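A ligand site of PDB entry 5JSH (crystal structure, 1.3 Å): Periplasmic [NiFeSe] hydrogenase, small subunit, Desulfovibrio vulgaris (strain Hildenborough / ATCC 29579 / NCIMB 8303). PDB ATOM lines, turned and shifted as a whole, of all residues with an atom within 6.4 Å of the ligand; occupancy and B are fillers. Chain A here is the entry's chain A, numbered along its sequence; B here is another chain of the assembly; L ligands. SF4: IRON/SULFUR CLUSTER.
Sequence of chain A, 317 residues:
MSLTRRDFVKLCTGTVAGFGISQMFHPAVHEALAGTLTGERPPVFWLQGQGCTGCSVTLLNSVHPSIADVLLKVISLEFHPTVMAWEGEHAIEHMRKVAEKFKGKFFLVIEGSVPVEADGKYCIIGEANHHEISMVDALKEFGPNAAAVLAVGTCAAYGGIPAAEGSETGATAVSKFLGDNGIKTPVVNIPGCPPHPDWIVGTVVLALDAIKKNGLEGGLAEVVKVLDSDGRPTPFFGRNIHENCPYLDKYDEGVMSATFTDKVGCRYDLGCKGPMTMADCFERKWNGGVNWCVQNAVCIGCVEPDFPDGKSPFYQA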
ATOM      1  N   GLN A  50      -9.108   1.109   9.351  1.00  0.00           N
ATOM      2  CA  GLN A  50     -10.225   1.988   9.691  1.00  0.00           C
ATOM      3  C   GLN A  50     -11.509   1.446   9.045  1.00  0.00           C
ATOM      4  O   GLN A  50     -12.052   2.023   8.117  1.00  0.00           O
ATOM      5  CB  GLN A  50      -9.948   3.404   9.233  1.00  0.00           C
ATOM      6  CG  GLN A  50      -8.834   4.106   9.976  1.00  0.00           C
ATOM      7  CD  GLN A  50      -8.463   5.413   9.322  1.00  0.00           C
ATOM      8  OE1 GLN A  50      -8.067   5.437   8.152  1.00  0.00           O
ATOM      9  NE2 GLN A  50      -8.611   6.513  10.053  1.00  0.00           N
ATOM     10  N   GLY A  51     -11.945   0.294   9.551  1.00  0.00           N
ATOM     11  CA  GLY A  51     -13.143  -0.380   9.089  1.00  0.00           C
ATOM     12  C   GLY A  51     -14.256  -0.278  10.128  1.00  0.00           C
ATOM     13  O   GLY A  51     -14.043   0.102  11.280  1.00  0.00           O
ATOM     14  N   CYS A  52     -15.466  -0.645   9.687  1.00  0.00           N
ATOM     15  CA  CYS A  52     -16.625  -0.708  10.587  1.00  0.00           C
ATOM     16  C   CYS A  52     -17.064  -2.138  10.867  1.00  0.00           C
ATOM     17  O   CYS A  52     -18.077  -2.343  11.535  1.00  0.00           O
ATOM     18  CB  CYS A  52     -17.806   0.089  10.008  1.00  0.00           C
ATOM     19  SG  CYS A  52     -18.769  -0.761   8.722  1.00  0.00           S
ATOM     20  N   THR A  53     -16.349  -3.133  10.353  1.00  0.00           N
ATOM     21  CA  THR A  53     -16.644  -4.558  10.478  1.00  0.00           C
ATOM     22  C   THR A  53     -17.809  -4.952   9.553  1.00  0.00           C
ATOM     23  O   THR A  53     -18.194  -6.133   9.515  1.00  0.00           O
ATOM     24  CB  THR A  53     -16.784  -4.972  11.956  1.00  0.00           C
ATOM     25  OG1 THR A  53     -15.592  -4.542  12.624  1.00  0.00           O
ATOM     26  CG2 THR A  53     -16.905  -6.480  12.144  1.00  0.00           C
ATOM     27  N   GLY A  54     -18.332  -4.019   8.773  1.00  0.00           N
ATOM     28  CA  GLY A  54     -19.415  -4.360   7.863  1.00  0.00           C
ATOM     29  C   GLY A  54     -19.000  -5.279   6.749  1.00  0.00           C
ATOM     30  O   GLY A  54     -19.835  -6.030   6.217  1.00  0.00           O
ATOM     31  N   CYS A  55     -17.737  -5.244   6.365  1.00  0.00           N
ATOM     32  CA  CYS A  55     -17.255  -6.130   5.317  1.00  0.00           C
ATOM     33  C   CYS A  55     -17.119  -7.569   5.825  1.00  0.00           C
ATOM     34  O   CYS A  55     -17.354  -8.524   5.072  1.00  0.00           O
ATOM     35  CB  CYS A  55     -15.974  -5.542   4.704  1.00  0.00           C
ATOM     36  SG  CYS A  55     -16.239  -3.990   3.712  1.00  0.00           S
ATOM     37  N   SER A  56     -16.816  -7.765   7.124  1.00  0.00           N
ATOM     38  CA  SER A  56     -16.876  -9.085   7.743  1.00  0.00           C
ATOM     39  C   SER A  56     -18.326  -9.551   7.870  1.00  0.00           C
ATOM     40  O   SER A  56     -18.647 -10.706   7.570  1.00  0.00           O
ATOM     41  CB  SER A  56     -16.220  -9.043   9.125  1.00  0.00           C
ATOM     42  OG  SER A  56     -14.812  -8.916   9.036  1.00  0.00           O
ATOM     43  N   GLU A 111      -9.627  -4.803   5.377  1.00  0.00           N
ATOM     44  CA  GLU A 111     -10.935  -4.174   5.602  1.00  0.00           C
ATOM     45  C   GLU A 111     -10.674  -2.836   6.269  1.00  0.00           C
ATOM     46  O   GLU A 111     -10.084  -2.802   7.361  1.00  0.00           O
ATOM     47  CB  GLU A 111     -11.797  -5.073   6.512  1.00  0.00           C
ATOM     48  CG  GLU A 111     -13.105  -4.441   7.079  1.00  0.00           C
ATOM     49  CD  GLU A 111     -14.047  -5.427   7.808  1.00  0.00           C
ATOM     50  OE1 GLU A 111     -13.563  -6.467   8.332  1.00  0.00           O
ATOM     51  OE2 GLU A 111     -15.270  -5.135   7.900  1.00  0.00           O
ATOM     52  N   GLY A 112     -11.119  -1.723   5.659  1.00  0.00           N
ATOM     53  CA  GLY A 112     -10.861  -0.403   6.184  1.00  0.00           C
ATOM     54  C   GLY A 112      -9.684   0.268   5.507  1.00  0.00           C
ATOM     55  O   GLY A 112      -8.840  -0.375   4.881  1.00  0.00           O
ATOM     56  N   SER A 113      -9.611   1.597   5.676  1.00  0.00           N
ATOM     57  CA  SER A 113      -8.503   2.377   5.151  1.00  0.00           C
ATOM     58  C   SER A 113      -7.302   2.340   6.090  1.00  0.00           C
ATOM     59  O   SER A 113      -7.382   1.855   7.232  1.00  0.00           O
ATOM     60  CB  SER A 113      -8.933   3.822   4.880  1.00  0.00           C
ATOM     61  OG  SER A 113      -9.540   4.412   6.014  1.00  0.00           O
ATOM     62  N   VAL A 152     -10.996  -5.291   0.483  1.00  0.00           N
ATOM     63  CA  VAL A 152     -12.428  -5.550   0.575  1.00  0.00           C
ATOM     64  C   VAL A 152     -13.119  -4.314   1.139  1.00  0.00           C
ATOM     65  O   VAL A 152     -12.733  -3.812   2.206  1.00  0.00           O
ATOM     66  CB  VAL A 152     -12.682  -6.806   1.439  1.00  0.00           C
ATOM     67  CG1 VAL A 152     -14.155  -6.992   1.715  1.00  0.00           C
ATOM     68  CG2 VAL A 152     -12.103  -8.038   0.740  1.00  0.00           C
ATOM     69  N   GLY A 153     -14.111  -3.825   0.423  1.00  0.00           N
ATOM     70  CA  GLY A 153     -14.847  -2.654   0.799  1.00  0.00           C
ATOM     71  C   GLY A 153     -14.266  -1.386   0.190  1.00  0.00           C
ATOM     72  O   GLY A 153     -13.079  -1.288  -0.115  1.00  0.00           O
ATOM     73  N   THR A 154     -15.141  -0.395   0.050  1.00  0.00           N
ATOM     74  CA  THR A 154     -14.737   0.879  -0.510  1.00  0.00           C
ATOM     75  C   THR A 154     -13.684   1.607   0.318  1.00  0.00           C
ATOM     76  O   THR A 154     -12.833   2.298  -0.251  1.00  0.00           O
ATOM     77  CB  THR A 154     -15.993   1.700  -0.744  1.00  0.00           C
ATOM     78  OG1 THR A 154     -16.722   1.024  -1.779  1.00  0.00           O
ATOM     79  CG2 THR A 154     -15.661   3.118  -1.184  1.00  0.00           C
ATOM     80  N   CYS A 155     -13.698   1.475   1.653  1.00  0.00           N
ATOM     81  CA  CYS A 155     -12.651   2.111   2.452  1.00  0.00           C
ATOM     82  C   CYS A 155     -11.266   1.598   2.034  1.00  0.00           C
ATOM     83  O   CYS A 155     -10.352   2.391   1.742  1.00  0.00           O
ATOM     84  CB  CYS A 155     -12.873   1.818   3.943  1.00  0.00           C
ATOM     85  SG  CYS A 155     -14.365   2.418   4.709  1.00  0.00           S
ATOM     86  N   ALA A 156     -11.083   0.292   2.030  1.00  0.00           N
ATOM     87  CA  ALA A 156      -9.797  -0.287   1.671  1.00  0.00           C
ATOM     88  C   ALA A 156      -9.476  -0.021   0.200  1.00  0.00           C
ATOM     89  O   ALA A 156      -8.317   0.253  -0.162  1.00  0.00           O
ATOM     90  CB  ALA A 156      -9.811  -1.778   1.974  1.00  0.00           C
ATOM     91  N   ILE A 161     -15.403   6.544   3.330  1.00  0.00           N
ATOM     92  CA  ILE A 161     -15.838   7.556   4.297  1.00  0.00           C
ATOM     93  C   ILE A 161     -14.686   8.059   5.149  1.00  0.00           C
ATOM     94  O   ILE A 161     -14.605   9.269   5.373  1.00  0.00           O
ATOM     95  CB  ILE A 161     -17.069   7.067   5.085  1.00  0.00           C
ATOM     96  CG1 ILE A 161     -18.287   7.047   4.143  1.00  0.00           C
ATOM     97  CG2 ILE A 161     -17.364   7.980   6.276  1.00  0.00           C
ATOM     98  CD1 ILE A 161     -19.455   6.284   4.652  1.00  0.00           C
ATOM     99  N   PRO A 162     -13.756   7.222   5.636  1.00  0.00           N
ATOM    100  CA  PRO A 162     -12.661   7.763   6.470  1.00  0.00           C
ATOM    101  C   PRO A 162     -11.781   8.772   5.748  1.00  0.00           C
ATOM    102  O   PRO A 162     -11.120   9.575   6.415  1.00  0.00           O
ATOM    103  CB  PRO A 162     -11.879   6.516   6.891  1.00  0.00           C
ATOM    104  CG  PRO A 162     -12.906   5.422   6.877  1.00  0.00           C
ATOM    105  CD  PRO A 162     -13.779   5.747   5.689  1.00  0.00           C
ATOM    106  N   GLY A 192     -17.683  -1.614  -2.499  1.00  0.00           N
ATOM    107  CA  GLY A 192     -19.005  -1.667  -1.911  1.00  0.00           C
ATOM    108  C   GLY A 192     -18.932  -1.244  -0.462  1.00  0.00           C
ATOM    109  O   GLY A 192     -17.896  -1.400   0.193  1.00  0.00           O
ATOM    110  N   CYS A 193     -20.034  -0.695   0.066  1.00  0.00           N
ATOM    111  CA  CYS A 193     -20.053  -0.250   1.458  1.00  0.00           C
ATOM    112  C   CYS A 193     -21.363  -0.704   2.104  1.00  0.00           C
ATOM    113  O   CYS A 193     -22.325   0.073   2.263  1.00  0.00           O
ATOM    114  CB  CYS A 193     -19.863   1.261   1.513  1.00  0.00           C
ATOM    115  SG  CYS A 193     -19.531   1.945   3.155  1.00  0.00           S
ATOM    116  N   PRO A 194     -21.464  -2.002   2.433  1.00  0.00           N
ATOM    117  CA  PRO A 194     -20.460  -3.038   2.182  1.00  0.00           C
ATOM    118  C   PRO A 194     -20.585  -3.683   0.808  1.00  0.00           C
ATOM    119  O   PRO A 194     -21.610  -3.500   0.124  1.00  0.00           O
ATOM    120  CB  PRO A 194     -20.826  -4.114   3.206  1.00  0.00           C
ATOM    121  CG  PRO A 194     -22.334  -4.044   3.249  1.00  0.00           C
ATOM    122  CD  PRO A 194     -22.685  -2.570   3.018  1.00  0.00           C
ATOM    123  N   PRO A 195     -19.572  -4.449   0.403  1.00  0.00           N
ATOM    124  CA  PRO A 195     -19.750  -5.352  -0.754  1.00  0.00           C
ATOM    125  C   PRO A 195     -20.849  -6.364  -0.471  1.00  0.00           C
ATOM    126  O   PRO A 195     -21.174  -6.668   0.672  1.00  0.00           O
ATOM    127  CB  PRO A 195     -18.382  -6.061  -0.862  1.00  0.00           C
ATOM    128  CG  PRO A 195     -17.429  -5.224  -0.045  1.00  0.00           C
ATOM    129  CD  PRO A 195     -18.266  -4.654   1.054  1.00  0.00           C
ATOM    130  N   PHE A 307     -17.055   7.540  -3.783  1.00  0.00           N
ATOM    131  CA  PHE A 307     -17.987   7.411  -2.646  1.00  0.00           C
ATOM    132  C   PHE A 307     -17.265   7.760  -1.324  1.00  0.00           C
ATOM    133  O   PHE A 307     -16.212   7.210  -1.033  1.00  0.00           O
ATOM    134  CB  PHE A 307     -18.561   5.995  -2.568  1.00  0.00           C
ATOM    135  CG  PHE A 307     -19.528   5.794  -1.435  1.00  0.00           C
ATOM    136  CD1 PHE A 307     -20.858   6.163  -1.559  1.00  0.00           C
ATOM    137  CD2 PHE A 307     -19.107   5.236  -0.240  1.00  0.00           C
ATOM    138  CE1 PHE A 307     -21.745   5.973  -0.520  1.00  0.00           C
ATOM    139  CE2 PHE A 307     -19.993   5.056   0.809  1.00  0.00           C
ATOM    140  CZ  PHE A 307     -21.303   5.421   0.676  1.00  0.00           C
ATOM    141  N   ARG B  50     -11.694   7.481  13.402  1.00  0.00           N
ATOM    142  CA  ARG B  50     -12.073   7.972  12.078  1.00  0.00           C
ATOM    143  C   ARG B  50     -12.584   9.404  12.089  1.00  0.00           C
ATOM    144  O   ARG B  50     -12.311  10.151  11.150  1.00  0.00           O
ATOM    145  CB  ARG B  50     -13.117   7.037  11.439  1.00  0.00           C
ATOM    146  CG  ARG B  50     -12.477   5.722  10.979  1.00  0.00           C
ATOM    147  CD  ARG B  50     -13.474   4.599  10.741  1.00  0.00           C
ATOM    148  NE  ARG B  50     -14.198   4.279  11.961  1.00  0.00           N
ATOM    149  CZ  ARG B  50     -15.363   3.651  12.012  1.00  0.00           C
ATOM    150  NH1 ARG B  50     -15.933   3.216  10.897  1.00  0.00           N
ATOM    151  NH2 ARG B  50     -15.978   3.482  13.178  1.00  0.00           N
ATOM    152  N   PHE B  52     -16.066  10.698  12.547  1.00  0.00           N
ATOM    153  CA  PHE B  52     -17.362  10.967  11.913  1.00  0.00           C
ATOM    154  C   PHE B  52     -17.950  12.328  12.271  1.00  0.00           C
ATOM    155  O   PHE B  52     -18.611  12.945  11.441  1.00  0.00           O
ATOM    156  CB  PHE B  52     -18.349   9.844  12.256  1.00  0.00           C
ATOM    157  CG  PHE B  52     -18.150   8.612  11.438  1.00  0.00           C
ATOM    158  CD1 PHE B  52     -17.097   7.761  11.712  1.00  0.00           C
ATOM    159  CD2 PHE B  52     -18.976   8.320  10.373  1.00  0.00           C
ATOM    160  CE1 PHE B  52     -16.896   6.628  10.946  1.00  0.00           C
ATOM    161  CE2 PHE B  52     -18.798   7.200   9.617  1.00  0.00           C
ATOM    162  CZ  PHE B  52     -17.751   6.359   9.883  1.00  0.00           C
ATOM    163  N   ARG B  70     -21.964   3.823   8.898  1.00  0.00           N
ATOM    164  CA  ARG B  70     -20.614   3.308   8.695  1.00  0.00           C
ATOM    165  C   ARG B  70     -19.729   3.484   9.922  1.00  0.00           C
ATOM    166  O   ARG B  70     -18.561   3.097   9.890  1.00  0.00           O
ATOM    167  CB  ARG B  70     -20.004   3.955   7.445  1.00  0.00           C
ATOM    168  CG  ARG B  70     -20.535   3.354   6.149  1.00  0.00           C
ATOM    169  CD  ARG B  70     -21.944   3.759   5.785  1.00  0.00           C
ATOM    170  NE  ARG B  70     -22.316   3.115   4.526  1.00  0.00           N
ATOM    171  CZ  ARG B  70     -23.532   3.135   3.980  1.00  0.00           C
ATOM    172  NH1 ARG B  70     -24.509   3.831   4.535  1.00  0.00           N
ATOM    173  NH2 ARG B  70     -23.765   2.439   2.878  1.00  0.00           N
ATOM    174  N   ILE B  71     -20.268   4.037  11.004  1.00  0.00           N
ATOM    175  CA  ILE B  71     -19.609   3.914  12.277  1.00  0.00           C
ATOM    176  C   ILE B  71     -19.424   2.450  12.652  1.00  0.00           C
ATOM    177  O   ILE B  71     -18.405   2.097  13.252  1.00  0.00           O
ATOM    178  CB  ILE B  71     -20.384   4.679  13.376  1.00  0.00           C
ATOM    179  CG1 ILE B  71     -20.252   6.183  13.160  1.00  0.00           C
ATOM    180  CG2 ILE B  71     -19.930   4.276  14.773  1.00  0.00           C
ATOM    181  CD1 ILE B  71     -21.236   7.010  13.937  1.00  0.00           C
ATOM    182  N   GLY B  73     -20.772  -1.600  11.337  1.00  0.00           N
ATOM    183  CA  GLY B  73     -21.501  -2.539  10.505  1.00  0.00           C
ATOM    184  C   GLY B  73     -22.216  -3.668  11.219  1.00  0.00           C
ATOM    185  O   GLY B  73     -22.918  -4.463  10.571  1.00  0.00           O
ATOM    186  N   PRO B 181     -25.547  -5.321   5.978  1.00  0.00           N
ATOM    187  CA  PRO B 181     -25.371  -4.029   6.652  1.00  0.00           C
ATOM    188  C   PRO B 181     -25.720  -2.811   5.807  1.00  0.00           C
ATOM    189  O   PRO B 181     -25.690  -2.853   4.579  1.00  0.00           O
ATOM    190  CB  PRO B 181     -23.869  -3.994   6.963  1.00  0.00           C
ATOM    191  CG  PRO B 181     -23.453  -5.410   7.030  1.00  0.00           C
ATOM    192  CD  PRO B 181     -24.291  -6.092   5.957  1.00  0.00           C
ATOM    193  N   HIS B 182     -26.105  -1.746   6.529  1.00  0.00           N
ATOM    194  CA  HIS B 182     -26.268  -0.378   6.035  1.00  0.00           C
ATOM    195  C   HIS B 182     -27.582  -0.227   5.279  1.00  0.00           C
ATOM    196  O   HIS B 182     -27.628  -0.227   4.041  1.00  0.00           O
ATOM    197  CB  HIS B 182     -25.048   0.118   5.253  1.00  0.00           C
ATOM    198  CG  HIS B 182     -23.789   0.060   6.056  1.00  0.00           C
ATOM    199  ND1 HIS B 182     -23.795   0.144   7.438  1.00  0.00           N
ATOM    200  CD2 HIS B 182     -22.499  -0.120   5.697  1.00  0.00           C
ATOM    201  CE1 HIS B 182     -22.560   0.036   7.888  1.00  0.00           C
ATOM    202  NE2 HIS B 182     -21.752  -0.121   6.849  1.00  0.00           N
HETATM  203 FE1  SF4 L   1     -17.597  -0.482   6.762  1.00  0.00          FE
HETATM  204 FE2  SF4 L   1     -15.676   0.603   5.097  1.00  0.00          FE
HETATM  205 FE3  SF4 L   1     -18.191   0.402   4.271  1.00  0.00          FE
HETATM  206 FE4  SF4 L   1     -16.782  -1.968   4.632  1.00  0.00          FE
HETATM  207  S1  SF4 L   1     -16.354  -0.297   3.114  1.00  0.00           S
HETATM  208  S2  SF4 L   1     -18.956  -1.530   5.212  1.00  0.00           S
HETATM  209  S3  SF4 L   1     -15.436  -1.303   6.395  1.00  0.00           S
HETATM  210  S4  SF4 L   1     -17.485   1.676   6.067  1.00  0.00           S
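The backbone NH (N) of Cys 155 lies close to a sulfur (S1) of the ligand (3.5 Å). SG of Cys 155 binds FE2 of the ligand. The side-chain sulfur (SG) of Cys 55 is bound to an iron atom (FE4) of the ligand, at 2.3 Å. The backbone NH (N) of Cys 52 of chain A lies close to a sulfur (S3) of the ligand (3.4 Å). An iron atom (FE1) of the ligand is bound by the side-chain sulfur (SG) of Cys 52 of chain A. SG of Cys 193 is bound to FE3 of the ligand (2.3 Å). A sulfur (S1) of the ligand sits close to the backbone NH (N) of Thr 154 (3.3 Å). A sulfur (S2) of the ligand lies close to a ring nitrogen (NE2) of His 182 of chain B, 3.5 Å away.
OE2 of Glu 111 is in hydrogen-bond range of N of Cys 55, at 2.9 Å. SG of Cys 52 of chain A sits close to NE2 of His 182 of chain B (3.6 Å). SG of Cys 52 of chain A lies close to N of Gly 54. N of Gly 73 of chain B sits at hydrogen-bond distance from O of Cys 52 of chain A (2.8 Å). The backbone carbonyl oxygen of Cys 193 lies within hydrogen-bond range of the guanidinium group of Arg 70 of chain B, 2.8 Å away. The side-chain hydroxyl (OG1) of Thr 154 is in hydrogen-bond range of the backbone NH (N) of Gly 192, at 2.9 Å. The side-chain carboxylate of Glu 111 lies close to the backbone NH of Thr 53. The side-chain carboxylate (OE1) of Glu 111 lies within hydrogen-bond range of the side-chain hydroxyl (OG) of Ser 56, 2.8 Å away.
S1 of the ligand sits close to O of Gly 192, 3.5 Å away. S2 of the ligand lies close to N of Pro 194 (3.8 Å). Merely in contact with the ligand: Arg 70 of chain B (3.5 Å), Gly 153 (3.6 Å), Gly 51 (3.7 Å), Gly 54 (3.9 Å) and Glu 111 (3.97 Å). Hydrophobic or aromatic side chains that line the ligand: Pro 194 and His 182 of chain B. Within 4 Å of the ligand: Gly 51, Cys 52 of chain A, Gly 54, Cys 55, Glu 111, Gly 153, Thr 154, Cys 155, Gly 192, Cys 193, Pro 194, Arg 70 of chain B and His 182 of chain B.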
